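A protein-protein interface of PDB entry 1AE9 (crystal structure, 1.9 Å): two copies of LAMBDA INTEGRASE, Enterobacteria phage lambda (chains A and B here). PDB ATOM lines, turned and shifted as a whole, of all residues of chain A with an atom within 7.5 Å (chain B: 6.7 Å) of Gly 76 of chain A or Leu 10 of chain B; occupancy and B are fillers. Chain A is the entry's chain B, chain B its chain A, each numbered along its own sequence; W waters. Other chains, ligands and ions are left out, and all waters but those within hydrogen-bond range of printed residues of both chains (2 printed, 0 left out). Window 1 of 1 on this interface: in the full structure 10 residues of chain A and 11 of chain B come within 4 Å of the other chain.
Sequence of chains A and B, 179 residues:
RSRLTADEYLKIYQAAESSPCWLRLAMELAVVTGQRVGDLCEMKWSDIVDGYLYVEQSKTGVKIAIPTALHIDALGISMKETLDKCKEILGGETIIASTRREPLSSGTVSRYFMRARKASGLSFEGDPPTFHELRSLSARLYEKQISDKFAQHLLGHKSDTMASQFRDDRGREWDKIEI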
ATOM      1  N   TYR A   9      15.657  12.799  18.576  1.00  0.00           N
ATOM      2  CA  TYR A   9      14.432  12.937  17.795  1.00  0.00           C
ATOM      3  C   TYR A   9      14.487  14.255  17.022  1.00  0.00           C
ATOM      4  O   TYR A   9      14.134  14.308  15.846  1.00  0.00           O
ATOM      5  CB  TYR A   9      13.207  12.935  18.715  1.00  0.00           C
ATOM      6  CG  TYR A   9      11.903  13.405  18.069  1.00  0.00           C
ATOM      7  CD1 TYR A   9      11.646  14.766  17.874  1.00  0.00           C
ATOM      8  CD2 TYR A   9      10.915  12.492  17.689  1.00  0.00           C
ATOM      9  CE1 TYR A   9      10.451  15.206  17.323  1.00  0.00           C
ATOM     10  CE2 TYR A   9       9.704  12.931  17.137  1.00  0.00           C
ATOM     11  CZ  TYR A   9       9.487  14.288  16.961  1.00  0.00           C
ATOM     12  OH  TYR A   9       8.302  14.740  16.438  1.00  0.00           O
ATOM     13  N   LEU A  10      14.915  15.322  17.694  1.00  0.00           N
ATOM     14  CA  LEU A  10      15.008  16.640  17.069  1.00  0.00           C
ATOM     15  C   LEU A  10      15.971  16.646  15.884  1.00  0.00           C
ATOM     16  O   LEU A  10      15.660  17.232  14.842  1.00  0.00           O
ATOM     17  CB  LEU A  10      15.401  17.703  18.105  1.00  0.00           C
ATOM     18  CG  LEU A  10      14.344  17.920  19.203  1.00  0.00           C
ATOM     19  CD1 LEU A  10      14.925  18.696  20.375  1.00  0.00           C
ATOM     20  CD2 LEU A  10      13.123  18.633  18.630  1.00  0.00           C
ATOM     21  N   GLU A  28       5.471  12.981  14.835  1.00  0.00           N
ATOM     22  CA  GLU A  28       4.751  13.763  15.834  1.00  0.00           C
ATOM     23  C   GLU A  28       3.608  12.954  16.422  1.00  0.00           C
ATOM     24  O   GLU A  28       3.447  12.892  17.645  1.00  0.00           O
ATOM     25  CB  GLU A  28       4.180  15.029  15.205  1.00  0.00           C
ATOM     26  CG  GLU A  28       5.215  16.041  14.751  1.00  0.00           C
ATOM     27  CD  GLU A  28       4.589  17.244  14.073  1.00  0.00           C
ATOM     28  OE1 GLU A  28       3.346  17.331  14.016  1.00  0.00           O
ATOM     29  OE2 GLU A  28       5.339  18.112  13.583  1.00  0.00           O
ATOM     30  N   HIS A  71      -0.715  16.894  24.651  1.00  0.00           N
ATOM     31  CA  HIS A  71       0.472  17.566  24.147  1.00  0.00           C
ATOM     32  C   HIS A  71       1.714  17.092  24.875  1.00  0.00           C
ATOM     33  O   HIS A  71       1.645  16.672  26.024  1.00  0.00           O
ATOM     34  CB  HIS A  71       0.346  19.098  24.199  1.00  0.00           C
ATOM     35  CG  HIS A  71       0.055  19.652  25.560  1.00  0.00           C
ATOM     36  ND1 HIS A  71       1.035  20.183  26.374  1.00  0.00           N
ATOM     37  CD2 HIS A  71      -1.113  19.818  26.224  1.00  0.00           C
ATOM     38  CE1 HIS A  71       0.482  20.655  27.476  1.00  0.00           C
ATOM     39  NE2 HIS A  71      -0.821  20.446  27.410  1.00  0.00           N
ATOM     40  N   ILE A  72       2.829  17.074  24.157  1.00  0.00           N
ATOM     41  CA  ILE A  72       4.117  16.663  24.697  1.00  0.00           C
ATOM     42  C   ILE A  72       4.933  17.951  24.794  1.00  0.00           C
ATOM     43  O   ILE A  72       5.232  18.566  23.774  1.00  0.00           O
ATOM     44  CB  ILE A  72       4.798  15.624  23.745  1.00  0.00           C
ATOM     45  CG1 ILE A  72       4.304  14.211  24.070  1.00  0.00           C
ATOM     46  CG2 ILE A  72       6.321  15.680  23.844  1.00  0.00           C
ATOM     47  CD1 ILE A  72       4.862  13.643  25.358  1.00  0.00           C
ATOM     48  N   ASP A  73       5.284  18.360  26.011  1.00  0.00           N
ATOM     49  CA  ASP A  73       6.029  19.604  26.222  1.00  0.00           C
ATOM     50  C   ASP A  73       7.452  19.614  25.702  1.00  0.00           C
ATOM     51  O   ASP A  73       7.849  20.549  25.013  1.00  0.00           O
ATOM     52  CB  ASP A  73       6.043  20.006  27.705  1.00  0.00           C
ATOM     53  CG  ASP A  73       4.658  20.335  28.245  1.00  0.00           C
ATOM     54  OD1 ASP A  73       3.741  20.663  27.456  1.00  0.00           O
ATOM     55  OD2 ASP A  73       4.484  20.261  29.476  1.00  0.00           O
ATOM     56  N   ALA A  74       8.204  18.567  26.017  1.00  0.00           N
ATOM     57  CA  ALA A  74       9.603  18.457  25.609  1.00  0.00           C
ATOM     58  C   ALA A  74       9.868  18.662  24.128  1.00  0.00           C
ATOM     59  O   ALA A  74      10.907  19.206  23.750  1.00  0.00           O
ATOM     60  CB  ALA A  74      10.172  17.119  26.051  1.00  0.00           C
ATOM     61  N   LEU A  75       8.935  18.218  23.291  1.00  0.00           N
ATOM     62  CA  LEU A  75       9.082  18.338  21.842  1.00  0.00           C
ATOM     63  C   LEU A  75       8.134  19.352  21.223  1.00  0.00           C
ATOM     64  O   LEU A  75       8.126  19.522  20.009  1.00  0.00           O
ATOM     65  CB  LEU A  75       8.889  16.972  21.167  1.00  0.00           C
ATOM     66  CG  LEU A  75       9.931  15.908  21.524  1.00  0.00           C
ATOM     67  CD1 LEU A  75       9.574  14.587  20.864  1.00  0.00           C
ATOM     68  CD2 LEU A  75      11.318  16.369  21.095  1.00  0.00           C
ATOM     69  N   GLY A  76       7.348  20.030  22.056  1.00  0.00           N
ATOM     70  CA  GLY A  76       6.414  21.019  21.551  1.00  0.00           C
ATOM     71  C   GLY A  76       5.424  20.449  20.549  1.00  0.00           C
ATOM     72  O   GLY A  76       5.233  21.015  19.467  1.00  0.00           O
ATOM     73  N   ILE A  77       4.796  19.329  20.898  1.00  0.00           N
ATOM     74  CA  ILE A  77       3.814  18.703  20.014  1.00  0.00           C
ATOM     75  C   ILE A  77       2.413  18.814  20.598  1.00  0.00           C
ATOM     76  O   ILE A  77       2.173  18.414  21.746  1.00  0.00           O
ATOM     77  CB  ILE A  77       4.103  17.195  19.796  1.00  0.00           C
ATOM     78  CG1 ILE A  77       5.483  16.986  19.178  1.00  0.00           C
ATOM     79  CG2 ILE A  77       3.050  16.586  18.880  1.00  0.00           C
ATOM     80  CD1 ILE A  77       5.977  15.550  19.289  1.00  0.00           C
ATOM     81  N   SER A  78       1.501  19.385  19.821  1.00  0.00           N
ATOM     82  CA  SER A  78       0.105  19.502  20.218  1.00  0.00           C
ATOM     83  C   SER A  78      -0.600  18.468  19.345  1.00  0.00           C
ATOM     84  O   SER A  78      -0.477  18.521  18.118  1.00  0.00           O
ATOM     85  CB  SER A  78      -0.417  20.898  19.893  1.00  0.00           C
ATOM     86  OG  SER A  78      -1.838  20.929  19.859  1.00  0.00           O
ATOM     87  N   MET A  79      -1.322  17.526  19.948  1.00  0.00           N
ATOM     88  CA  MET A  79      -2.000  16.502  19.156  1.00  0.00           C
ATOM     89  C   MET A  79      -2.991  17.107  18.172  1.00  0.00           C
ATOM     90  O   MET A  79      -3.041  16.704  17.007  1.00  0.00           O
ATOM     91  CB  MET A  79      -2.696  15.476  20.047  1.00  0.00           C
ATOM     92  CG  MET A  79      -3.368  14.341  19.262  1.00  0.00           C
ATOM     93  SD  MET A  79      -3.902  12.998  20.320  1.00  0.00           S
ATOM     94  CE  MET A  79      -4.970  12.101  19.207  1.00  0.00           C
ATOM     95  N   LYS A  80      -3.761  18.091  18.628  1.00  0.00           N
ATOM     96  CA  LYS A  80      -4.731  18.747  17.761  1.00  0.00           C
ATOM     97  C   LYS A  80      -4.029  19.437  16.592  1.00  0.00           C
ATOM     98  O   LYS A  80      -4.458  19.330  15.449  1.00  0.00           O
ATOM     99  CB  LYS A  80      -5.550  19.767  18.556  1.00  0.00           C
ATOM    100  CG  LYS A  80      -6.731  20.342  17.788  1.00  0.00           C
ATOM    101  CD  LYS A  80      -7.710  19.240  17.418  1.00  0.00           C
ATOM    102  CE  LYS A  80      -9.018  19.799  16.926  1.00  0.00           C
ATOM    103  NZ  LYS A  80      -8.830  20.591  15.688  1.00  0.00           N
ATOM    104  N   GLU A  81      -2.932  20.127  16.877  1.00  0.00           N
ATOM    105  CA  GLU A  81      -2.182  20.836  15.844  1.00  0.00           C
ATOM    106  C   GLU A  81      -1.611  19.862  14.816  1.00  0.00           C
ATOM    107  O   GLU A  81      -1.630  20.133  13.619  1.00  0.00           O
ATOM    108  CB  GLU A  81      -1.067  21.666  16.483  1.00  0.00           C
ATOM    109  CG  GLU A  81      -0.556  22.794  15.602  1.00  0.00           C
ATOM    110  CD  GLU A  81       0.714  22.460  14.846  1.00  0.00           C
ATOM    111  OE1 GLU A  81       1.349  21.416  15.124  1.00  0.00           O
ATOM    112  OE2 GLU A  81       1.089  23.276  13.981  1.00  0.00           O
ATOM    113  N   THR A  82      -1.104  18.729  15.284  1.00  0.00           N
ATOM    114  CA  THR A  82      -0.560  17.711  14.393  1.00  0.00           C
ATOM    115  C   THR A  82      -1.691  17.141  13.530  1.00  0.00           C
ATOM    116  O   THR A  82      -1.536  16.983  12.319  1.00  0.00           O
ATOM    117  CB  THR A  82       0.135  16.599  15.197  1.00  0.00           C
ATOM    118  OG1 THR A  82       1.323  17.136  15.792  1.00  0.00           O
ATOM    119  CG2 THR A  82       0.493  15.401  14.306  1.00  0.00           C
ATOM    120  N   LYS A  85      -2.613  19.485  10.834  1.00  0.00           N
ATOM    121  CA  LYS A  85      -1.619  19.422   9.770  1.00  0.00           C
ATOM    122  C   LYS A  85      -1.816  18.175   8.910  1.00  0.00           C
ATOM    123  O   LYS A  85      -1.691  18.238   7.691  1.00  0.00           O
ATOM    124  CB  LYS A  85      -0.194  19.471  10.337  1.00  0.00           C
ATOM    125  CG  LYS A  85       0.223  20.857  10.831  1.00  0.00           C
ATOM    126  CD  LYS A  85       1.740  20.987  10.994  1.00  0.00           C
ATOM    127  CE  LYS A  85       2.281  20.047  12.065  1.00  0.00           C
ATOM    128  NZ  LYS A  85       3.766  20.147  12.200  1.00  0.00           N
ATOM    129  N   LEU B   4       3.589  35.520  13.976  1.00  0.00           N
ATOM    130  CA  LEU B   4       3.981  34.227  14.524  1.00  0.00           C
ATOM    131  C   LEU B   4       2.819  33.276  14.287  1.00  0.00           C
ATOM    132  O   LEU B   4       1.697  33.568  14.684  1.00  0.00           O
ATOM    133  CB  LEU B   4       4.251  34.341  16.026  1.00  0.00           C
ATOM    134  CG  LEU B   4       4.833  33.100  16.706  1.00  0.00           C
ATOM    135  CD1 LEU B   4       6.286  32.921  16.294  1.00  0.00           C
ATOM    136  CD2 LEU B   4       4.708  33.239  18.219  1.00  0.00           C
ATOM    137  N   THR B   5       3.075  32.159  13.610  1.00  0.00           N
ATOM    138  CA  THR B   5       2.021  31.182  13.339  1.00  0.00           C
ATOM    139  C   THR B   5       1.914  30.191  14.497  1.00  0.00           C
ATOM    140  O   THR B   5       2.786  30.152  15.376  1.00  0.00           O
ATOM    141  CB  THR B   5       2.284  30.393  12.025  1.00  0.00           C
ATOM    142  OG1 THR B   5       3.430  29.546  12.182  1.00  0.00           O
ATOM    143  CG2 THR B   5       2.522  31.346  10.872  1.00  0.00           C
ATOM    144  N   ALA B   6       0.858  29.384  14.490  1.00  0.00           N
ATOM    145  CA  ALA B   6       0.660  28.382  15.529  1.00  0.00           C
ATOM    146  C   ALA B   6       1.795  27.354  15.538  1.00  0.00           C
ATOM    147  O   ALA B   6       2.268  26.966  16.608  1.00  0.00           O
ATOM    148  CB  ALA B   6      -0.683  27.683  15.346  1.00  0.00           C
ATOM    149  N   ASP B   7       2.227  26.906  14.356  1.00  0.00           N
ATOM    150  CA  ASP B   7       3.307  25.920  14.271  1.00  0.00           C
ATOM    151  C   ASP B   7       4.628  26.520  14.793  1.00  0.00           C
ATOM    152  O   ASP B   7       5.404  25.837  15.472  1.00  0.00           O
ATOM    153  CB  ASP B   7       3.462  25.389  12.829  1.00  0.00           C
ATOM    154  CG  ASP B   7       4.245  24.063  12.757  1.00  0.00           C
ATOM    155  OD1 ASP B   7       3.774  23.038  13.297  1.00  0.00           O
ATOM    156  OD2 ASP B   7       5.334  24.035  12.149  1.00  0.00           O
ATOM    157  N   GLU B   8       4.857  27.802  14.511  1.00  0.00           N
ATOM    158  CA  GLU B   8       6.066  28.486  14.964  1.00  0.00           C
ATOM    159  C   GLU B   8       6.048  28.640  16.481  1.00  0.00           C
ATOM    160  O   GLU B   8       7.092  28.522  17.126  1.00  0.00           O
ATOM    161  CB  GLU B   8       6.217  29.844  14.269  1.00  0.00           C
ATOM    162  CG  GLU B   8       6.596  29.716  12.794  1.00  0.00           C
ATOM    163  CD  GLU B   8       6.552  31.032  12.024  1.00  0.00           C
ATOM    164  OE1 GLU B   8       5.870  31.979  12.469  1.00  0.00           O
ATOM    165  OE2 GLU B   8       7.192  31.114  10.954  1.00  0.00           O
ATOM    166  N   TYR B   9       4.865  28.881  17.045  1.00  0.00           N
ATOM    167  CA  TYR B   9       4.695  29.003  18.495  1.00  0.00           C
ATOM    168  C   TYR B   9       5.170  27.709  19.159  1.00  0.00           C
ATOM    169  O   TYR B   9       5.830  27.738  20.204  1.00  0.00           O
ATOM    170  CB  TYR B   9       3.214  29.249  18.837  1.00  0.00           C
ATOM    171  CG  TYR B   9       2.815  28.982  20.282  1.00  0.00           C
ATOM    172  CD1 TYR B   9       2.644  27.677  20.746  1.00  0.00           C
ATOM    173  CD2 TYR B   9       2.620  30.030  21.186  1.00  0.00           C
ATOM    174  CE1 TYR B   9       2.297  27.414  22.075  1.00  0.00           C
ATOM    175  CE2 TYR B   9       2.267  29.778  22.526  1.00  0.00           C
ATOM    176  CZ  TYR B   9       2.111  28.465  22.958  1.00  0.00           C
ATOM    177  OH  TYR B   9       1.779  28.178  24.264  1.00  0.00           O
ATOM    178  N   LEU B  10       4.811  26.572  18.564  1.00  0.00           N
ATOM    179  CA  LEU B  10       5.199  25.271  19.103  1.00  0.00           C
ATOM    180  C   LEU B  10       6.707  25.014  19.028  1.00  0.00           C
ATOM    181  O   LEU B  10       7.272  24.361  19.915  1.00  0.00           O
ATOM    182  CB  LEU B  10       4.401  24.145  18.421  1.00  0.00           C
ATOM    183  CG  LEU B  10       2.906  24.108  18.789  1.00  0.00           C
ATOM    184  CD1 LEU B  10       2.162  23.063  17.971  1.00  0.00           C
ATOM    185  CD2 LEU B  10       2.736  23.825  20.269  1.00  0.00           C
ATOM    186  N   LYS B  11       7.367  25.526  17.989  1.00  0.00           N
ATOM    187  CA  LYS B  11       8.823  25.350  17.858  1.00  0.00           C
ATOM    188  C   LYS B  11       9.518  26.125  18.985  1.00  0.00           C
ATOM    189  O   LYS B  11      10.445  25.620  19.627  1.00  0.00           O
ATOM    190  CB  LYS B  11       9.322  25.849  16.496  1.00  0.00           C
ATOM    191  CG  LYS B  11       8.649  25.208  15.293  1.00  0.00           C
ATOM    192  CD  LYS B  11       8.796  23.691  15.293  1.00  0.00           C
ATOM    193  CE  LYS B  11       8.232  23.089  14.010  1.00  0.00           C
ATOM    194  NZ  LYS B  11       8.252  21.608  14.042  1.00  0.00           N
ATOM    195  N   ILE B  12       9.059  27.350  19.225  1.00  0.00           N
ATOM    196  CA  ILE B  12       9.612  28.192  20.282  1.00  0.00           C
ATOM    197  C   ILE B  12       9.305  27.567  21.644  1.00  0.00           C
ATOM    198  O   ILE B  12      10.157  27.557  22.542  1.00  0.00           O
ATOM    199  CB  ILE B  12       9.028  29.623  20.213  1.00  0.00           C
ATOM    200  CG1 ILE B  12       9.440  30.287  18.891  1.00  0.00           C
ATOM    201  CG2 ILE B  12       9.482  30.440  21.427  1.00  0.00           C
ATOM    202  CD1 ILE B  12       8.827  31.665  18.636  1.00  0.00           C
ATOM    203  N   TYR B  13       8.088  27.038  21.788  1.00  0.00           N
ATOM    204  CA  TYR B  13       7.651  26.379  23.017  1.00  0.00           C
ATOM    205  C   TYR B  13       8.607  25.226  23.327  1.00  0.00           C
ATOM    206  O   TYR B  13       9.027  25.055  24.471  1.00  0.00           O
ATOM    207  CB  TYR B  13       6.216  25.856  22.850  1.00  0.00           C
ATOM    208  CG  TYR B  13       5.564  25.353  24.123  1.00  0.00           C
ATOM    209  CD1 TYR B  13       5.777  24.053  24.571  1.00  0.00           C
ATOM    210  CD2 TYR B  13       4.733  26.181  24.875  1.00  0.00           C
ATOM    211  CE1 TYR B  13       5.180  23.590  25.737  1.00  0.00           C
ATOM    212  CE2 TYR B  13       4.133  25.727  26.042  1.00  0.00           C
ATOM    213  CZ  TYR B  13       4.362  24.434  26.467  1.00  0.00           C
ATOM    214  OH  TYR B  13       3.783  23.982  27.636  1.00  0.00           O
ATOM    215  N   GLN B  14       8.945  24.442  22.300  1.00  0.00           N
ATOM    216  CA  GLN B  14       9.869  23.313  22.442  1.00  0.00           C
ATOM    217  C   GLN B  14      11.224  23.846  22.893  1.00  0.00           C
ATOM    218  O   GLN B  14      11.840  23.317  23.825  1.00  0.00           O
ATOM    219  CB  GLN B  14      10.029  22.583  21.095  1.00  0.00           C
ATOM    220  CG  GLN B  14      10.955  21.357  21.101  1.00  0.00           C
ATOM    221  CD  GLN B  14      12.447  21.702  21.182  1.00  0.00           C
ATOM    222  OE1 GLN B  14      12.954  22.487  20.384  1.00  0.00           O
ATOM    223  NE2 GLN B  14      13.148  21.114  22.148  1.00  0.00           N
ATOM    224  N   ALA B  15      11.687  24.887  22.203  1.00  0.00           N
ATOM    225  CA  ALA B  15      12.977  25.510  22.481  1.00  0.00           C
ATOM    226  C   ALA B  15      13.062  26.075  23.896  1.00  0.00           C
ATOM    227  O   ALA B  15      14.155  26.221  24.438  1.00  0.00           O
ATOM    228  CB  ALA B  15      13.262  26.596  21.453  1.00  0.00           C
ATOM    229  N   ARG B  24       7.057  29.129  29.416  1.00  0.00           N
ATOM    230  CA  ARG B  24       6.007  28.380  28.729  1.00  0.00           C
ATOM    231  C   ARG B  24       4.621  28.767  29.237  1.00  0.00           C
ATOM    232  O   ARG B  24       3.675  28.892  28.451  1.00  0.00           O
ATOM    233  CB  ARG B  24       6.222  26.871  28.886  1.00  0.00           C
ATOM    234  CG  ARG B  24       7.323  26.321  27.989  1.00  0.00           C
ATOM    235  CD  ARG B  24       7.475  24.819  28.143  1.00  0.00           C
ATOM    236  NE  ARG B  24       8.348  24.250  27.117  1.00  0.00           N
ATOM    237  CZ  ARG B  24       9.041  23.119  27.250  1.00  0.00           C
ATOM    238  NH1 ARG B  24       8.979  22.417  28.373  1.00  0.00           N
ATOM    239  NH2 ARG B  24       9.793  22.681  26.250  1.00  0.00           N
ATOM    240  N   MET B  27       3.634  32.141  27.946  1.00  0.00           N
ATOM    241  CA  MET B  27       3.289  31.995  26.522  1.00  0.00           C
ATOM    242  C   MET B  27       1.851  31.499  26.376  1.00  0.00           C
ATOM    243  O   MET B  27       1.060  32.058  25.604  1.00  0.00           O
ATOM    244  CB  MET B  27       4.246  31.027  25.808  1.00  0.00           C
ATOM    245  CG  MET B  27       5.613  31.625  25.479  1.00  0.00           C
ATOM    246  SD  MET B  27       6.805  30.434  24.839  1.00  0.00           S
ATOM    247  CE  MET B  27       6.018  30.042  23.231  1.00  0.00           C
ATOM    248  N   ALA B  74      -6.621  25.137  18.615  1.00  0.00           N
ATOM    249  CA  ALA B  74      -5.507  24.920  17.693  1.00  0.00           C
ATOM    250  C   ALA B  74      -4.186  24.480  18.330  1.00  0.00           C
ATOM    251  O   ALA B  74      -3.390  23.777  17.700  1.00  0.00           O
ATOM    252  CB  ALA B  74      -5.289  26.161  16.833  1.00  0.00           C
ATOM    253  N   LEU B  75      -3.964  24.874  19.579  1.00  0.00           N
ATOM    254  CA  LEU B  75      -2.729  24.538  20.277  1.00  0.00           C
ATOM    255  C   LEU B  75      -2.942  23.686  21.518  1.00  0.00           C
ATOM    256  O   LEU B  75      -1.981  23.317  22.193  1.00  0.00           O
ATOM    257  CB  LEU B  75      -1.975  25.819  20.643  1.00  0.00           C
ATOM    258  CG  LEU B  75      -1.451  26.625  19.455  1.00  0.00           C
ATOM    259  CD1 LEU B  75      -0.976  27.987  19.922  1.00  0.00           C
ATOM    260  CD2 LEU B  75      -0.326  25.862  18.775  1.00  0.00           C
HETATM  261  O   HOH W   1       6.651  19.402  15.730  1.00  0.00           O
HETATM  262  O   HOH W   2       6.758  21.668  11.522  1.00  0.00           O
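NE2 of Gln 14 of chain B touches CD1 of Leu 10 of chain A, at 3.5 Å.
Leu 75 of chain A touches Gln 14 of chain B.
Leu 10 of chain B touches Gly 76 of chain A.
Gln 14 of chain B touches Gly 76 of chain A.
Leu 10 of chain B touches Ser 78 of chain A (CD1 to CB, 3.9 Å).
Ser 78 of chain A touches Ala 74 of chain B (OG to O, 3.9 Å).
Glu 81 of chain A touches Leu 10 of chain B.
Glu 81 of chain A touches Ala 74 of chain B (CB to O, 3.4 Å).
Of the 16 printed residues of chain B, 7 touch a printed residue of chain A.
Printed residues of chain B that touch a printed residue of chain A: Asp 7, Leu 10, Tyr 13, Gln 14, Arg 24, Ala 74 and Leu 75.
Hydrophobic or aromatic side chains of chain B within 4 Å of the printed part of chain A: Leu 10 and Tyr 13.
Hydrophobic or aromatic side chains of chain A within 4 Å of the printed part of chain B: Leu 10.
Along chain A the printed residues that touch a printed residue of chain B span positions 10 to 85.
The backbone carbonyl oxygen (O) of Ser 78 of chain A is in hydrogen-bond range of the side-chain hydroxyl (OG1) of Thr 82 of chain A, 3.3 Å away.
O of Gln 14 of chain B lies within hydrogen-bond range of NH2 of Arg 24 of chain B (3.2 Å).
The side-chain amino group of Lys 85 of chain A is in salt-bridge range of the side-chain carboxylate of Glu 28 of chain A, 2.9 Å away.
The side-chain hydroxyl of Ser 78 of chain A sits at hydrogen-bond distance from the backbone NH of Glu 81 of chain A, 3.3 Å away.
NE of Arg 24 of chain B is in hydrogen-bond range of O of Tyr 13 of chain B (2.8 Å).
The side-chain carboxylate (OD1) of Asp 73 of chain A sits at hydrogen-bond distance from a ring nitrogen (ND1) of His 71 of chain A (3.0 Å).
Water W1 lies within hydrogen-bond range of the side-chain carboxylate of Glu 28 of chain A (2.8 Å) and the side-chain amino group of Lys 11 of chain B (3.2 Å).
Water W2 lies within hydrogen-bond range of the side-chain carboxylate (OD2) of Asp 7 of chain B (2.8 Å), the side-chain amino group (NZ) of Lys 11 of chain B (2.9 Å) and the side-chain amino group (NZ) of Lys 85 of chain A (3.4 Å).
Of the printed residues of chain B, Asp 73 of chain A touches Tyr 13 and Arg 24.
Printed residues of chain B within 4 Å of Leu 75 of chain A: Gln 14.
Gly 76 of chain A touches just these residues of chain B: Leu 10 and Gln 14.
Printed residues of chain B within 4 Å of Glu 81 of chain A: Asp 7, Leu 10 and Ala 74.
Printed residues of chain B within 4 Å of Lys 85 of chain A: Asp 7 (3.1 Å).
Tyr 9 of chain B touches none of the printed residues of chain A.
Printed residues of chain A within 4 Å of Leu 10 of chain B: Gly 76, Ser 78 and Glu 81.
Ala 15 of chain B touches none of the printed residues of chain A.
The nearest residue of chain B that does not touch Gly 76 of chain A is Tyr 13 of chain B (4.3 Å).
The nearest printed residue of chain B that does not touch Ala 74 of chain A is Arg 24 of chain B (4.3 Å).
Positions printed for both chains: 9, 10, 74 and 75.
Of the 14 pairs that touch across the chains among the printed residues, none has its exchanged pair printed and touching as well.
The side-chain hydroxyl (OG) of Ser 78 of chain A is in hydrogen-bond range of the backbone carbonyl oxygen (O) of Leu 75 of chain B (3.3 Å).
The side-chain carboxylate of Asp 7 of chain B lies within salt-bridge range of the side-chain amino group of Lys 85 of chain A (3.1 Å).
OH of Tyr 13 of chain B sits at hydrogen-bond distance from OD1 of Asp 73 of chain A (3.3 Å).
The side-chain carboxylate (OD1) of Asp 7 of chain B lies close to the side-chain carboxylate (OE2) of Glu 81 of chain A.
The side-chain amide nitrogen (NE2) of Gln 14 of chain B lies within hydrogen-bond range of the backbone carbonyl oxygen (O) of Ala 74 of chain A, at 3.4 Å.
The guanidinium group (NH2) of Arg 24 of chain B sits at hydrogen-bond distance from the backbone carbonyl oxygen (O) of Asp 73 of chain A (3.1 Å).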
